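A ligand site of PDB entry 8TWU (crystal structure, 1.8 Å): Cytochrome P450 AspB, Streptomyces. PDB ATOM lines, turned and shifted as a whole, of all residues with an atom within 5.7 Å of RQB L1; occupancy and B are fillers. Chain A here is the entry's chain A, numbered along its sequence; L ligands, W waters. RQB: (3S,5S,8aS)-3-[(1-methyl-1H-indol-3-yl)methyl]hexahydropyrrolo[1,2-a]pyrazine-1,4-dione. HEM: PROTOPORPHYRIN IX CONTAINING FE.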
ATOM      1  N   GLN A  75     -24.323   4.988 -35.266  1.00  0.00           N
ATOM      2  CA  GLN A  75     -25.236   5.163 -34.137  1.00  0.00           C
ATOM      3  C   GLN A  75     -25.317   6.608 -33.662  1.00  0.00           C
ATOM      4  O   GLN A  75     -26.345   7.009 -33.102  1.00  0.00           O
ATOM      5  CB  GLN A  75     -24.796   4.310 -32.943  1.00  0.00           C
ATOM      6  CG  GLN A  75     -23.467   4.765 -32.302  1.00  0.00           C
ATOM      7  CD  GLN A  75     -22.857   3.689 -31.413  1.00  0.00           C
ATOM      8  OE1 GLN A  75     -23.281   3.496 -30.274  1.00  0.00           O
ATOM      9  NE2 GLN A  75     -21.851   2.976 -31.934  1.00  0.00           N
ATOM     10  N   GLU A  76     -24.266   7.391 -33.871  1.00  0.00           N
ATOM     11  CA  GLU A  76     -24.149   8.740 -33.331  1.00  0.00           C
ATOM     12  C   GLU A  76     -24.773   9.768 -34.277  1.00  0.00           C
ATOM     13  O   GLU A  76     -24.789   9.563 -35.491  1.00  0.00           O
ATOM     14  CB  GLU A  76     -22.674   9.072 -33.084  1.00  0.00           C
ATOM     15  CG  GLU A  76     -21.822   9.093 -34.320  1.00  0.00           C
ATOM     16  CD  GLU A  76     -21.150   7.763 -34.636  1.00  0.00           C
ATOM     17  OE1 GLU A  76     -21.634   6.716 -34.175  1.00  0.00           O
ATOM     18  OE2 GLU A  76     -20.114   7.770 -35.343  1.00  0.00           O
ATOM     19  N   LEU A  80     -18.054  11.976 -35.879  1.00  0.00           N
ATOM     20  CA  LEU A  80     -17.160  12.326 -34.781  1.00  0.00           C
ATOM     21  C   LEU A  80     -15.801  12.775 -35.346  1.00  0.00           C
ATOM     22  O   LEU A  80     -14.781  12.128 -35.189  1.00  0.00           O
ATOM     23  CB  LEU A  80     -16.982  11.135 -33.833  1.00  0.00           C
ATOM     24  CG  LEU A  80     -18.260  10.502 -33.280  1.00  0.00           C
ATOM     25  CD1 LEU A  80     -17.911   9.318 -32.379  1.00  0.00           C
ATOM     26  CD2 LEU A  80     -19.119  11.554 -32.536  1.00  0.00           C
ATOM     27  N   PHE A 177     -24.946  11.634 -27.711  1.00  0.00           N
ATOM     28  CA  PHE A 177     -26.119  11.294 -28.515  1.00  0.00           C
ATOM     29  C   PHE A 177     -27.113  12.449 -28.600  1.00  0.00           C
ATOM     30  O   PHE A 177     -27.891  12.509 -29.557  1.00  0.00           O
ATOM     31  CB  PHE A 177     -26.826  10.054 -27.946  1.00  0.00           C
ATOM     32  CG  PHE A 177     -26.092   8.760 -28.206  1.00  0.00           C
ATOM     33  CD1 PHE A 177     -26.068   8.214 -29.492  1.00  0.00           C
ATOM     34  CD2 PHE A 177     -25.397   8.119 -27.195  1.00  0.00           C
ATOM     35  CE1 PHE A 177     -25.382   7.032 -29.759  1.00  0.00           C
ATOM     36  CE2 PHE A 177     -24.707   6.935 -27.439  1.00  0.00           C
ATOM     37  CZ  PHE A 177     -24.697   6.396 -28.728  1.00  0.00           C
ATOM     38  N   VAL A 239     -10.098  11.901 -26.701  1.00  0.00           N
ATOM     39  CA  VAL A 239     -11.358  11.163 -26.576  1.00  0.00           C
ATOM     40  C   VAL A 239     -11.113   9.798 -25.936  1.00  0.00           C
ATOM     41  O   VAL A 239     -11.992   9.273 -25.238  1.00  0.00           O
ATOM     42  CB  VAL A 239     -12.082  11.022 -27.928  1.00  0.00           C
ATOM     43  CG1 VAL A 239     -12.367  12.395 -28.552  1.00  0.00           C
ATOM     44  CG2 VAL A 239     -11.295  10.140 -28.879  1.00  0.00           C
ATOM     45  N   ALA A 240      -9.926   9.207 -26.117  1.00  0.00           N
ATOM     46  CA  ALA A 240      -9.637   7.899 -25.524  1.00  0.00           C
ATOM     47  C   ALA A 240      -9.323   7.969 -24.028  1.00  0.00           C
ATOM     48  O   ALA A 240      -9.632   7.025 -23.290  1.00  0.00           O
ATOM     49  CB  ALA A 240      -8.451   7.234 -26.259  1.00  0.00           C
ATOM     50  N   THR A 244     -13.247   9.055 -20.683  1.00  0.00           N
ATOM     51  CA  THR A 244     -13.281   7.670 -20.227  1.00  0.00           C
ATOM     52  C   THR A 244     -12.769   7.580 -18.799  1.00  0.00           C
ATOM     53  O   THR A 244     -13.444   7.021 -17.910  1.00  0.00           O
ATOM     54  CB  THR A 244     -12.412   6.815 -21.161  1.00  0.00           C
ATOM     55  OG1 THR A 244     -11.140   7.447 -21.278  1.00  0.00           O
ATOM     56  CG2 THR A 244     -13.058   6.725 -22.547  1.00  0.00           C
ATOM     57  N   LEU A 286     -19.887   2.121 -18.208  1.00  0.00           N
ATOM     58  CA  LEU A 286     -19.224   3.347 -18.654  1.00  0.00           C
ATOM     59  C   LEU A 286     -19.936   3.987 -19.839  1.00  0.00           C
ATOM     60  O   LEU A 286     -20.338   5.156 -19.773  1.00  0.00           O
ATOM     61  CB  LEU A 286     -17.747   3.062 -19.011  1.00  0.00           C
ATOM     62  CG  LEU A 286     -16.999   4.326 -19.475  1.00  0.00           C
ATOM     63  CD1 LEU A 286     -17.097   5.463 -18.445  1.00  0.00           C
ATOM     64  CD2 LEU A 286     -15.543   3.972 -19.767  1.00  0.00           C
ATOM     65  N   SER A 287     -20.101   3.242 -20.919  1.00  0.00           N
ATOM     66  CA  SER A 287     -20.594   3.799 -22.174  1.00  0.00           C
ATOM     67  C   SER A 287     -22.102   3.615 -22.328  1.00  0.00           C
ATOM     68  O   SER A 287     -22.664   2.584 -21.923  1.00  0.00           O
ATOM     69  CB  SER A 287     -19.874   3.151 -23.365  1.00  0.00           C
ATOM     70  OG  SER A 287     -20.311   3.725 -24.577  1.00  0.00           O
ATOM     71  N   THR A 288     -22.745   4.616 -22.925  1.00  0.00           N
ATOM     72  CA  THR A 288     -24.147   4.538 -23.299  1.00  0.00           C
ATOM     73  C   THR A 288     -24.340   4.109 -24.755  1.00  0.00           C
ATOM     74  O   THR A 288     -25.465   3.921 -25.196  1.00  0.00           O
ATOM     75  CB  THR A 288     -24.840   5.891 -23.073  1.00  0.00           C
ATOM     76  OG1 THR A 288     -24.234   6.860 -23.934  1.00  0.00           O
ATOM     77  CG2 THR A 288     -24.704   6.336 -21.613  1.00  0.00           C
ATOM     78  N   GLY A 289     -23.248   4.012 -25.518  1.00  0.00           N
ATOM     79  CA  GLY A 289     -23.286   3.485 -26.858  1.00  0.00           C
ATOM     80  C   GLY A 289     -22.590   2.141 -26.948  1.00  0.00           C
ATOM     81  O   GLY A 289     -22.385   1.436 -25.948  1.00  0.00           O
ATOM     82  N   SER A 290     -22.187   1.779 -28.175  1.00  0.00           N
ATOM     83  CA  SER A 290     -21.588   0.461 -28.404  1.00  0.00           C
ATOM     84  C   SER A 290     -20.315   0.587 -29.226  1.00  0.00           C
ATOM     85  O   SER A 290     -20.176   1.492 -30.051  1.00  0.00           O
ATOM     86  CB  SER A 290     -22.549  -0.492 -29.158  1.00  0.00           C
ATOM     87  OG  SER A 290     -23.698  -0.778 -28.394  1.00  0.00           O
ATOM     88  N   VAL A 291     -19.371  -0.335 -28.984  1.00  0.00           N
ATOM     89  CA  VAL A 291     -18.252  -0.455 -29.920  1.00  0.00           C
ATOM     90  C   VAL A 291     -18.844  -0.926 -31.253  1.00  0.00           C
ATOM     91  O   VAL A 291     -19.916  -1.532 -31.294  1.00  0.00           O
ATOM     92  CB  VAL A 291     -17.183  -1.428 -29.406  1.00  0.00           C
ATOM     93  CG1 VAL A 291     -16.544  -0.923 -28.104  1.00  0.00           C
ATOM     94  CG2 VAL A 291     -17.776  -2.809 -29.190  1.00  0.00           C
ATOM     95  N   LYS A 292     -18.149  -0.620 -32.358  1.00  0.00           N
ATOM     96  CA  LYS A 292     -18.766  -0.969 -33.624  1.00  0.00           C
ATOM     97  C   LYS A 292     -17.713  -1.379 -34.659  1.00  0.00           C
ATOM     98  O   LYS A 292     -16.553  -0.949 -34.608  1.00  0.00           O
ATOM     99  CB  LYS A 292     -19.628   0.193 -34.163  1.00  0.00           C
ATOM    100  CG  LYS A 292     -18.834   1.314 -34.826  1.00  0.00           C
ATOM    101  CD  LYS A 292     -18.124   2.219 -33.826  1.00  0.00           C
ATOM    102  CE  LYS A 292     -17.812   3.583 -34.468  1.00  0.00           C
ATOM    103  NZ  LYS A 292     -16.968   4.425 -33.588  1.00  0.00           N
ATOM    104  N   LEU A 316     -20.884  -3.235 -24.524  1.00  0.00           N
ATOM    105  CA  LEU A 316     -20.034  -3.872 -23.527  1.00  0.00           C
ATOM    106  C   LEU A 316     -20.740  -3.964 -22.186  1.00  0.00           C
ATOM    107  O   LEU A 316     -20.511  -4.924 -21.431  1.00  0.00           O
ATOM    108  CB  LEU A 316     -18.708  -3.102 -23.401  1.00  0.00           C
ATOM    109  CG  LEU A 316     -17.986  -2.862 -24.742  1.00  0.00           C
ATOM    110  CD1 LEU A 316     -16.699  -2.029 -24.533  1.00  0.00           C
ATOM    111  CD2 LEU A 316     -17.665  -4.176 -25.455  1.00  0.00           C
ATOM    112  N   GLU A 317     -21.607  -2.995 -21.882  1.00  0.00           N
ATOM    113  CA  GLU A 317     -22.362  -3.008 -20.632  1.00  0.00           C
ATOM    114  C   GLU A 317     -23.320  -4.190 -20.598  1.00  0.00           C
ATOM    115  O   GLU A 317     -23.365  -4.940 -19.612  1.00  0.00           O
ATOM    116  CB  GLU A 317     -23.113  -1.682 -20.463  1.00  0.00           C
ATOM    117  CG  GLU A 317     -22.204  -0.435 -20.186  1.00  0.00           C
ATOM    118  CD  GLU A 317     -21.285  -0.069 -21.355  1.00  0.00           C
ATOM    119  OE1 GLU A 317     -21.654  -0.261 -22.522  1.00  0.00           O
ATOM    120  OE2 GLU A 317     -20.155   0.395 -21.089  1.00  0.00           O
ATOM    121  N   GLY A 343     -14.865  -4.707 -20.049  1.00  0.00           N
ATOM    122  CA  GLY A 343     -14.680  -3.289 -19.755  1.00  0.00           C
ATOM    123  C   GLY A 343     -13.638  -2.608 -20.632  1.00  0.00           C
ATOM    124  O   GLY A 343     -13.714  -1.405 -20.878  1.00  0.00           O
ATOM    125  N   PHE A 390     -21.776   9.963 -24.291  1.00  0.00           N
ATOM    126  CA  PHE A 390     -21.304   8.607 -24.585  1.00  0.00           C
ATOM    127  C   PHE A 390     -20.755   7.935 -23.329  1.00  0.00           C
ATOM    128  O   PHE A 390     -20.973   6.739 -23.113  1.00  0.00           O
ATOM    129  CB  PHE A 390     -20.175   8.616 -25.622  1.00  0.00           C
ATOM    130  CG  PHE A 390     -20.602   9.009 -27.021  1.00  0.00           C
ATOM    131  CD1 PHE A 390     -21.946   9.080 -27.361  1.00  0.00           C
ATOM    132  CD2 PHE A 390     -19.629   9.335 -27.979  1.00  0.00           C
ATOM    133  CE1 PHE A 390     -22.325   9.460 -28.659  1.00  0.00           C
ATOM    134  CE2 PHE A 390     -19.997   9.721 -29.283  1.00  0.00           C
ATOM    135  CZ  PHE A 390     -21.352   9.787 -29.617  1.00  0.00           C
ATOM    136  N   PHE A 391     -20.007   8.679 -22.528  1.00  0.00           N
ATOM    137  CA  PHE A 391     -19.362   8.138 -21.330  1.00  0.00           C
ATOM    138  C   PHE A 391     -20.055   8.750 -20.118  1.00  0.00           C
ATOM    139  O   PHE A 391     -19.824   9.913 -19.786  1.00  0.00           O
ATOM    140  CB  PHE A 391     -17.874   8.432 -21.386  1.00  0.00           C
ATOM    141  CG  PHE A 391     -17.202   7.808 -22.601  1.00  0.00           C
ATOM    142  CD1 PHE A 391     -17.230   6.436 -22.761  1.00  0.00           C
ATOM    143  CD2 PHE A 391     -16.607   8.594 -23.587  1.00  0.00           C
ATOM    144  CE1 PHE A 391     -16.633   5.813 -23.864  1.00  0.00           C
ATOM    145  CE2 PHE A 391     -16.011   7.994 -24.707  1.00  0.00           C
ATOM    146  CZ  PHE A 391     -16.033   6.596 -24.842  1.00  0.00           C
HETATM  147  C10 RQB L   1     -19.530   5.820 -28.670  1.00  0.00           C
HETATM  148  C13 RQB L   1     -19.165   5.318 -30.991  1.00  0.00           C
HETATM  149  C15 RQB L   1     -17.863   4.049 -29.513  1.00  0.00           C
HETATM  150  C17 RQB L   1     -15.624   2.755 -25.653  1.00  0.00           C
HETATM  151  C20 RQB L   1     -13.590   3.618 -23.946  1.00  0.00           C
HETATM  152  C21 RQB L   1     -14.645   2.857 -23.430  1.00  0.00           C
HETATM  153  C22 RQB L   1     -15.693   2.423 -24.296  1.00  0.00           C
HETATM  154  C01 RQB L   1     -17.280   1.111 -22.785  1.00  0.00           C
HETATM  155  C03 RQB L   1     -17.507   1.516 -25.223  1.00  0.00           C
HETATM  156  C04 RQB L   1     -16.779   2.183 -26.246  1.00  0.00           C
HETATM  157  C05 RQB L   1     -17.133   2.309 -27.754  1.00  0.00           C
HETATM  158  C06 RQB L   1     -17.565   3.805 -27.971  1.00  0.00           C
HETATM  159  C08 RQB L   1     -19.853   5.123 -27.413  1.00  0.00           C
HETATM  160  C11 RQB L   1     -20.752   6.090 -29.334  1.00  0.00           C
HETATM  161  C12 RQB L   1     -20.389   6.248 -30.802  1.00  0.00           C
HETATM  162  C18 RQB L   1     -14.561   3.513 -26.174  1.00  0.00           C
HETATM  163  C19 RQB L   1     -13.533   3.956 -25.305  1.00  0.00           C
HETATM  164  N02 RQB L   1     -16.838   1.663 -24.080  1.00  0.00           N
HETATM  165  N07 RQB L   1     -18.795   3.990 -26.955  1.00  0.00           N
HETATM  166  N14 RQB L   1     -18.766   4.983 -29.728  1.00  0.00           N
HETATM  167  O09 RQB L   1     -20.799   5.351 -26.751  1.00  0.00           O
HETATM  168  O16 RQB L   1     -17.317   3.459 -30.376  1.00  0.00           O
HETATM  169  CHA HEM L   2     -10.107   1.677 -26.908  1.00  0.00           C
HETATM  170  CHB HEM L   2      -6.551   4.482 -25.185  1.00  0.00           C
HETATM  171  CHC HEM L   2      -8.676   4.540 -20.841  1.00  0.00           C
HETATM  172  CHD HEM L   2     -11.890   1.303 -22.442  1.00  0.00           C
HETATM  173  C1A HEM L   2      -9.022   2.519 -26.837  1.00  0.00           C
HETATM  174  C2A HEM L   2      -8.270   2.977 -27.979  1.00  0.00           C
HETATM  175  C3A HEM L   2      -7.270   3.757 -27.516  1.00  0.00           C
HETATM  176  C4A HEM L   2      -7.371   3.806 -26.065  1.00  0.00           C
HETATM  177  CMA HEM L   2      -6.187   4.474 -28.346  1.00  0.00           C
HETATM  178  CAA HEM L   2      -8.627   2.571 -29.432  1.00  0.00           C
HETATM  179  CBA HEM L   2      -7.921   1.257 -29.766  1.00  0.00           C
HETATM  180  CGA HEM L   2      -8.245   0.701 -31.139  1.00  0.00           C
HETATM  181  O1A HEM L   2      -9.352   0.994 -31.673  1.00  0.00           O
HETATM  182  O2A HEM L   2      -7.420  -0.079 -31.676  1.00  0.00           O
HETATM  183  C1B HEM L   2      -6.802   4.748 -23.864  1.00  0.00           C
HETATM  184  C2B HEM L   2      -5.968   5.550 -22.989  1.00  0.00           C
HETATM  185  C3B HEM L   2      -6.575   5.578 -21.785  1.00  0.00           C
HETATM  186  C4B HEM L   2      -7.785   4.773 -21.862  1.00  0.00           C
HETATM  187  CMB HEM L   2      -4.657   6.244 -23.470  1.00  0.00           C
HETATM  188  CAB HEM L   2      -6.149   6.262 -20.462  1.00  0.00           C
HETATM  189  CBB HEM L   2      -4.948   6.849 -20.350  1.00  0.00           C
HETATM  190  C1C HEM L   2      -9.740   3.675 -20.872  1.00  0.00           C
HETATM  191  C2C HEM L   2     -10.643   3.347 -19.774  1.00  0.00           C
HETATM  192  C3C HEM L   2     -11.516   2.450 -20.247  1.00  0.00           C
HETATM  193  C4C HEM L   2     -11.203   2.188 -21.631  1.00  0.00           C
HETATM  194  CMC HEM L   2     -10.597   3.947 -18.330  1.00  0.00           C
HETATM  195  CAC HEM L   2     -12.689   1.733 -19.530  1.00  0.00           C
HETATM  196  CBC HEM L   2     -12.848   1.877 -18.209  1.00  0.00           C
HETATM  197  C1D HEM L   2     -11.685   1.114 -23.782  1.00  0.00           C
HETATM  198  C2D HEM L   2     -12.432   0.204 -24.637  1.00  0.00           C
HETATM  199  C3D HEM L   2     -11.955   0.305 -25.876  1.00  0.00           C
HETATM  200  C4D HEM L   2     -10.868   1.269 -25.841  1.00  0.00           C
HETATM  201  CMD HEM L   2     -13.607  -0.711 -24.180  1.00  0.00           C
HETATM  202  CAD HEM L   2     -12.408  -0.533 -27.108  1.00  0.00           C
HETATM  203  CBD HEM L   2     -13.213   0.239 -28.129  1.00  0.00           C
HETATM  204  CGD HEM L   2     -13.443  -0.641 -29.346  1.00  0.00           C
HETATM  205  O1D HEM L   2     -13.665  -0.049 -30.419  1.00  0.00           O
HETATM  206  O2D HEM L   2     -13.409  -1.911 -29.267  1.00  0.00           O
HETATM  207  NA  HEM L   2      -8.455   3.049 -25.691  1.00  0.00           N
HETATM  208  NB  HEM L   2      -7.883   4.275 -23.142  1.00  0.00           N
HETATM  209  NC  HEM L   2     -10.116   2.943 -21.984  1.00  0.00           N
HETATM  210  ND  HEM L   2     -10.719   1.743 -24.553  1.00  0.00           N
HETATM  211 FE   HEM L   2      -9.163   2.809 -23.803  1.00  0.00          FE
HETATM  212  C10 RQB L   3     -11.133  10.396 -33.491  1.00  0.00           C
HETATM  213  C13 RQB L   3     -13.184  11.209 -32.594  1.00  0.00           C
HETATM  214  C15 RQB L   3     -13.275   8.938 -33.272  1.00  0.00           C
HETATM  215  C17 RQB L   3     -13.703   6.806 -30.627  1.00  0.00           C
HETATM  216  C20 RQB L   3     -15.154   7.375 -28.272  1.00  0.00           C
HETATM  217  C21 RQB L   3     -13.829   6.959 -28.177  1.00  0.00           C
HETATM  218  C22 RQB L   3     -13.114   6.680 -29.371  1.00  0.00           C
HETATM  219  C01 RQB L   3     -10.901   6.031 -28.422  1.00  0.00           C
HETATM  220  C03 RQB L   3     -11.528   6.128 -30.834  1.00  0.00           C
HETATM  221  C04 RQB L   3     -12.688   6.458 -31.593  1.00  0.00           C
HETATM  222  C05 RQB L   3     -12.857   6.406 -33.141  1.00  0.00           C
HETATM  223  C06 RQB L   3     -12.416   7.742 -33.913  1.00  0.00           C
HETATM  224  C08 RQB L   3     -10.171   9.268 -33.599  1.00  0.00           C
HETATM  225  C11 RQB L   3     -10.749  11.425 -32.648  1.00  0.00           C
HETATM  226  C12 RQB L   3     -12.046  12.270 -32.500  1.00  0.00           C
HETATM  227  C18 RQB L   3     -15.054   7.223 -30.704  1.00  0.00           C
HETATM  228  C19 RQB L   3     -15.772   7.493 -29.524  1.00  0.00           C
HETATM  229  N02 RQB L   3     -11.814   6.278 -29.540  1.00  0.00           N
HETATM  230  N07 RQB L   3     -10.815   7.826 -33.838  1.00  0.00           N
HETATM  231  N14 RQB L   3     -12.601  10.078 -33.123  1.00  0.00           N
HETATM  232  O09 RQB L   3      -8.986   9.375 -33.580  1.00  0.00           O
HETATM  233  O16 RQB L   3     -14.399   8.767 -33.005  1.00  0.00           O
HETATM  234  O   HOH W   1     -15.615   0.998 -31.721  1.00  0.00           O
HETATM  235  O   HOH W   2     -10.659   4.632 -24.572  1.00  0.00           O
HETATM  236  O   HOH W   3     -20.368  -0.329 -24.956  1.00  0.00           O
HETATM  237  O   HOH W   4     -15.939   0.124 -19.787  1.00  0.00           O
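O09 of RQB L1 is in hydrogen-bond range of OG of Ser 287, 2.8 Å away.
An oxygen (O16) of RQB L1 is in hydrogen-bond range of the side-chain amino group (NZ) of Lys 292, at 3.4 Å.
N of Gly 289 lies within hydrogen-bond range of O09 of RQB L1 (3.1 Å).
The backbone carbonyl oxygen of Phe 390 is in hydrogen-bond range of the backbone NH of Thr 288, 2.8 Å away.
The side-chain carboxylate of Glu 317 sits at hydrogen-bond distance from the backbone NH of Leu 286 (3.4 Å).
The backbone NH (N) of Ser 290 sits at hydrogen-bond distance from the side-chain amide oxygen (OE1) of Gln 75 (2.9 Å).
The side-chain hydroxyl of Ser 287 lies within hydrogen-bond range of the backbone NH of Gly 289, 3.1 Å away.
The backbone NH of Ser 287 sits at hydrogen-bond distance from the side-chain carboxylate of Glu 317 (2.9 Å).
The backbone carbonyl oxygen of Ala 240 sits at hydrogen-bond distance from the side-chain hydroxyl of Thr 244, 2.5 Å away.
OG of Ser 287 sits close to O of Phe 390.
An oxygen (O16) of RQB L1 sits close to the backbone carbonyl oxygen (O) of Ser 290, at 3.5 Å.
CD of Gln 75 touches C12 of RQB L1, at 3.6 Å.
Glu 76 touches RQB L1 (OE1 to C12, 3.6 Å).
Thr 244 touches RQB L1.
CD2 of Leu 286 touches C21 of RQB L1 (3.9 Å).
Val 291 touches RQB L1 (CG1 to C05, 3.3 Å).
Leu 316 touches RQB L1 (CD1 to C01, 3.6 Å).
Glu 317 touches RQB L1 (OE2 to C01, 3.4 Å).
Phe 390 touches RQB L1 (CB to O09, 3.5 Å).
Phe 391 touches RQB L1.
Hydrophobic or aromatic side chains that line RQB L1: Leu 286, Val 291, Leu 316, Phe 390 and Phe 391.
Of the 19 residues printed, 13 come within 4 Å of RQB L1.
Water W1 lies within hydrogen-bond range of an oxygen (O1D) of HEM L2 (2.6 Å), the backbone NH of Lys 292 (3.1 Å) and an oxygen (O16) of RQB L1 (3.3 Å).
Water W3 lies within hydrogen-bond range of the side-chain carboxylate (OE1) of Glu 317 (2.8 Å), the backbone carbonyl oxygen (O) of Gly 289 (2.9 Å) and the backbone NH (N) of Leu 316 (3.0 Å).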
